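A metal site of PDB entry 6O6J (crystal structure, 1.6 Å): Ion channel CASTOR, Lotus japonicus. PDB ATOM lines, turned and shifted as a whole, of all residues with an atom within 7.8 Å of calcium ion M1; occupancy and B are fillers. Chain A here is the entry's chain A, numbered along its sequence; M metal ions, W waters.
Water W2 lies within hydrogen-bond range of OD2 of Asp 244 (2.6 Å), O of Ile 32 (2.8 Å) and N of Ser 36 (3.0 Å).
Calcium ion M1 is bound by water W1, the backbone carbonyl oxygen (O) of Ala 33, the side-chain carboxylate (OD1) of Asp 245, water W3, the side-chain hydroxyl (OG) of Ser 36, the side-chain carboxylate (OD1) of Asp 244 and water W2.
Calcium ion M1 has seven donor atoms within binding distance.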
ATOM      1  N   LEU A  30     -20.408   2.555  10.721  1.00  0.00           N
ATOM      2  CA  LEU A  30     -20.326   1.101  10.705  1.00  0.00           C
ATOM      3  C   LEU A  30     -20.894   0.541   9.413  1.00  0.00           C
ATOM      4  O   LEU A  30     -20.359  -0.439   8.880  1.00  0.00           O
ATOM      5  CB  LEU A  30     -21.029   0.508  11.921  1.00  0.00           C
ATOM      6  CG  LEU A  30     -20.345   0.802  13.252  1.00  0.00           C
ATOM      7  CD1 LEU A  30     -21.304   0.535  14.446  1.00  0.00           C
ATOM      8  CD2 LEU A  30     -19.054  -0.006  13.365  1.00  0.00           C
ATOM      9  N   ALA A  31     -21.947   1.180   8.875  1.00  0.00           N
ATOM     10  CA  ALA A  31     -22.484   0.767   7.566  1.00  0.00           C
ATOM     11  C   ALA A  31     -21.427   0.939   6.481  1.00  0.00           C
ATOM     12  O   ALA A  31     -21.245   0.041   5.626  1.00  0.00           O
ATOM     13  CB  ALA A  31     -23.731   1.584   7.255  1.00  0.00           C
ATOM     14  N   ILE A  32     -20.676   2.049   6.536  1.00  0.00           N
ATOM     15  CA  ILE A  32     -19.618   2.266   5.535  1.00  0.00           C
ATOM     16  C   ILE A  32     -18.511   1.219   5.686  1.00  0.00           C
ATOM     17  O   ILE A  32     -18.029   0.664   4.693  1.00  0.00           O
ATOM     18  CB  ILE A  32     -19.079   3.703   5.644  1.00  0.00           C
ATOM     19  CG1 ILE A  32     -20.174   4.738   5.326  1.00  0.00           C
ATOM     20  CG2 ILE A  32     -17.940   3.916   4.639  1.00  0.00           C
ATOM     21  CD1 ILE A  32     -19.798   6.173   5.829  1.00  0.00           C
ATOM     22  N   ALA A  33     -18.096   0.948   6.927  1.00  0.00           N
ATOM     23  CA  ALA A  33     -17.068  -0.066   7.168  1.00  0.00           C
ATOM     24  C   ALA A  33     -17.500  -1.450   6.698  1.00  0.00           C
ATOM     25  O   ALA A  33     -16.681  -2.227   6.189  1.00  0.00           O
ATOM     26  CB  ALA A  33     -16.701  -0.099   8.677  1.00  0.00           C
ATOM     27  N   ASN A  34     -18.791  -1.792   6.869  1.00  0.00           N
ATOM     28  CA  ASN A  34     -19.292  -3.111   6.497  1.00  0.00           C
ATOM     29  C   ASN A  34     -19.579  -3.239   4.999  1.00  0.00           C
ATOM     30  O   ASN A  34     -19.874  -4.350   4.563  1.00  0.00           O
ATOM     31  CB  ASN A  34     -20.611  -3.437   7.218  1.00  0.00           C
ATOM     32  CG  ASN A  34     -20.434  -3.757   8.713  1.00  0.00           C
ATOM     33  OD1 ASN A  34     -19.363  -4.152   9.171  1.00  0.00           O
ATOM     34  ND2 ASN A  34     -21.547  -3.629   9.463  1.00  0.00           N
ATOM     35  N   GLU A  35     -19.592  -2.145   4.253  1.00  0.00           N
ATOM     36  CA  GLU A  35     -20.072  -2.218   2.866  1.00  0.00           C
ATOM     37  C   GLU A  35     -19.269  -3.221   2.042  1.00  0.00           C
ATOM     38  O   GLU A  35     -19.849  -3.949   1.208  1.00  0.00           O
ATOM     39  CB  GLU A  35     -20.008  -0.841   2.232  1.00  0.00           C
ATOM     40  CG  GLU A  35     -20.607  -0.823   0.811  1.00  0.00           C
ATOM     41  CD  GLU A  35     -20.536   0.544   0.184  1.00  0.00           C
ATOM     42  OE1 GLU A  35     -19.637   1.332   0.562  1.00  0.00           O
ATOM     43  OE2 GLU A  35     -21.398   0.846  -0.670  1.00  0.00           O
ATOM     44  N   SER A  36     -17.946  -3.282   2.236  1.00  0.00           N
ATOM     45  CA  SER A  36     -17.091  -4.187   1.463  1.00  0.00           C
ATOM     46  C   SER A  36     -17.427  -5.656   1.675  1.00  0.00           C
ATOM     47  O   SER A  36     -17.072  -6.497   0.828  1.00  0.00           O
ATOM     48  CB  SER A  36     -15.631  -3.908   1.809  1.00  0.00           C
ATOM     49  OG  SER A  36     -15.388  -4.177   3.192  1.00  0.00           O
ATOM     50  N   LEU A  37     -18.074  -5.998   2.797  1.00  0.00           N
ATOM     51  CA  LEU A  37     -18.555  -7.351   3.055  1.00  0.00           C
ATOM     52  C   LEU A  37     -19.924  -7.623   2.459  1.00  0.00           C
ATOM     53  O   LEU A  37     -20.401  -8.748   2.569  1.00  0.00           O
ATOM     54  CB  LEU A  37     -18.654  -7.612   4.560  1.00  0.00           C
ATOM     55  CG  LEU A  37     -17.340  -7.297   5.267  1.00  0.00           C
ATOM     56  CD1 LEU A  37     -17.493  -7.292   6.788  1.00  0.00           C
ATOM     57  CD2 LEU A  37     -16.295  -8.279   4.833  1.00  0.00           C
ATOM     58  N   GLY A  38     -20.577  -6.621   1.890  1.00  0.00           N
ATOM     59  CA  GLY A  38     -21.976  -6.740   1.514  1.00  0.00           C
ATOM     60  C   GLY A  38     -22.955  -6.429   2.629  1.00  0.00           C
ATOM     61  O   GLY A  38     -24.148  -6.730   2.489  1.00  0.00           O
ATOM     62  N   PHE A 180     -14.821   6.433   7.867  1.00  0.00           N
ATOM     63  CA  PHE A 180     -14.626   5.381   6.880  1.00  0.00           C
ATOM     64  C   PHE A 180     -14.851   5.827   5.450  1.00  0.00           C
ATOM     65  O   PHE A 180     -14.472   5.085   4.534  1.00  0.00           O
ATOM     66  CB  PHE A 180     -15.494   4.159   7.197  1.00  0.00           C
ATOM     67  CG  PHE A 180     -14.877   3.272   8.266  1.00  0.00           C
ATOM     68  CD1 PHE A 180     -13.855   2.387   7.931  1.00  0.00           C
ATOM     69  CD2 PHE A 180     -15.242   3.390   9.616  1.00  0.00           C
ATOM     70  CE1 PHE A 180     -13.216   1.585   8.912  1.00  0.00           C
ATOM     71  CE2 PHE A 180     -14.602   2.593  10.589  1.00  0.00           C
ATOM     72  CZ  PHE A 180     -13.593   1.706  10.251  1.00  0.00           C
ATOM     73  N   GLU A 184      -8.334   5.424   5.263  1.00  0.00           N
ATOM     74  CA  GLU A 184      -8.169   5.343   6.720  1.00  0.00           C
ATOM     75  C   GLU A 184      -7.122   4.271   7.045  1.00  0.00           C
ATOM     76  O   GLU A 184      -6.609   3.596   6.150  1.00  0.00           O
ATOM     77  CB  GLU A 184      -9.530   5.079   7.401  1.00  0.00           C
ATOM     78  CG  GLU A 184     -10.269   3.782   6.894  1.00  0.00           C
ATOM     79  CD  GLU A 184     -11.150   3.985   5.669  1.00  0.00           C
ATOM     80  OE1 GLU A 184     -11.419   5.131   5.243  1.00  0.00           O
ATOM     81  OE2 GLU A 184     -11.587   2.951   5.097  1.00  0.00           O
ATOM     82  N   TYR A 186      -5.441   0.847   8.282  1.00  0.00           N
ATOM     83  CA  TYR A 186      -5.659  -0.594   8.351  1.00  0.00           C
ATOM     84  C   TYR A 186      -4.368  -1.299   8.743  1.00  0.00           C
ATOM     85  O   TYR A 186      -3.272  -0.895   8.350  1.00  0.00           O
ATOM     86  CB  TYR A 186      -6.133  -1.198   7.011  1.00  0.00           C
ATOM     87  CG  TYR A 186      -7.529  -0.746   6.670  1.00  0.00           C
ATOM     88  CD1 TYR A 186      -8.628  -1.342   7.267  1.00  0.00           C
ATOM     89  CD2 TYR A 186      -7.751   0.302   5.790  1.00  0.00           C
ATOM     90  CE1 TYR A 186      -9.934  -0.910   6.996  1.00  0.00           C
ATOM     91  CE2 TYR A 186      -9.060   0.742   5.489  1.00  0.00           C
ATOM     92  CZ  TYR A 186     -10.140   0.123   6.121  1.00  0.00           C
ATOM     93  OH  TYR A 186     -11.423   0.570   5.908  1.00  0.00           O
ATOM     94  N   GLU A 243      -7.990   2.772   1.041  1.00  0.00           N
ATOM     95  CA  GLU A 243      -9.401   3.111   0.842  1.00  0.00           C
ATOM     96  C   GLU A 243     -10.353   2.192   1.610  1.00  0.00           C
ATOM     97  O   GLU A 243     -11.414   2.648   2.090  1.00  0.00           O
ATOM     98  CB  GLU A 243      -9.727   3.073  -0.655  1.00  0.00           C
ATOM     99  CG  GLU A 243     -11.120   3.632  -0.923  1.00  0.00           C
ATOM    100  CD  GLU A 243     -11.405   3.825  -2.423  1.00  0.00           C
ATOM    101  OE1 GLU A 243     -11.123   2.908  -3.219  1.00  0.00           O
ATOM    102  OE2 GLU A 243     -11.917   4.910  -2.788  1.00  0.00           O
ATOM    103  N   ASP A 244     -10.012   0.912   1.738  1.00  0.00           N
ATOM    104  CA  ASP A 244     -10.851  -0.052   2.437  1.00  0.00           C
ATOM    105  C   ASP A 244      -9.938  -1.204   2.827  1.00  0.00           C
ATOM    106  O   ASP A 244      -8.773  -1.264   2.411  1.00  0.00           O
ATOM    107  CB  ASP A 244     -12.046  -0.489   1.549  1.00  0.00           C
ATOM    108  CG  ASP A 244     -13.328  -0.772   2.357  1.00  0.00           C
ATOM    109  OD1 ASP A 244     -13.250  -1.224   3.499  1.00  0.00           O
ATOM    110  OD2 ASP A 244     -14.447  -0.536   1.826  1.00  0.00           O
ATOM    111  N   ASP A 245     -10.480  -2.147   3.588  1.00  0.00           N
ATOM    112  CA  ASP A 245      -9.617  -3.200   4.108  1.00  0.00           C
ATOM    113  C   ASP A 245      -9.125  -4.134   3.018  1.00  0.00           C
ATOM    114  O   ASP A 245      -8.133  -4.840   3.232  1.00  0.00           O
ATOM    115  CB  ASP A 245     -10.352  -4.029   5.174  1.00  0.00           C
ATOM    116  CG  ASP A 245     -11.666  -4.619   4.659  1.00  0.00           C
ATOM    117  OD1 ASP A 245     -12.686  -3.903   4.656  1.00  0.00           O
ATOM    118  OD2 ASP A 245     -11.693  -5.805   4.226  1.00  0.00           O
ATOM    119  N   ASP A 246      -9.811  -4.148   1.880  1.00  0.00           N
ATOM    120  CA  ASP A 246      -9.568  -5.145   0.838  1.00  0.00           C
ATOM    121  C   ASP A 246      -9.137  -4.514  -0.495  1.00  0.00           C
ATOM    122  O   ASP A 246      -9.184  -5.195  -1.524  1.00  0.00           O
ATOM    123  CB  ASP A 246     -10.819  -5.995   0.634  1.00  0.00           C
ATOM    124  CG  ASP A 246     -12.042  -5.172   0.157  1.00  0.00           C
ATOM    125  OD1 ASP A 246     -11.989  -3.923   0.073  1.00  0.00           O
ATOM    126  OD2 ASP A 246     -13.095  -5.791  -0.156  1.00  0.00           O
ATOM    127  N   GLU A 457     -13.742  -1.358  14.949  1.00  0.00           N
ATOM    128  CA  GLU A 457     -13.376  -2.230  13.831  1.00  0.00           C
ATOM    129  C   GLU A 457     -11.996  -2.853  14.015  1.00  0.00           C
ATOM    130  O   GLU A 457     -11.782  -3.989  13.584  1.00  0.00           O
ATOM    131  CB  GLU A 457     -13.459  -1.426  12.519  1.00  0.00           C
ATOM    132  CG  GLU A 457     -14.905  -1.192  12.106  1.00  0.00           C
ATOM    133  CD  GLU A 457     -15.574  -2.490  11.689  1.00  0.00           C
ATOM    134  OE1 GLU A 457     -15.200  -3.079  10.640  1.00  0.00           O
ATOM    135  OE2 GLU A 457     -16.495  -2.933  12.406  1.00  0.00           O
HETATM  136 CA    CA M   1     -14.688  -2.609   4.923  1.00  0.00          CA
HETATM  137 CA    CA M   2     -12.808   4.029   3.329  1.00  0.00          CA
HETATM  138  O   HOH W   1     -13.682  -1.135   6.467  1.00  0.00           O
HETATM  139  O   HOH W   2     -16.278  -1.208   3.534  1.00  0.00           O
HETATM  140  O   HOH W   3     -14.929  -4.441   6.514  1.00  0.00           O
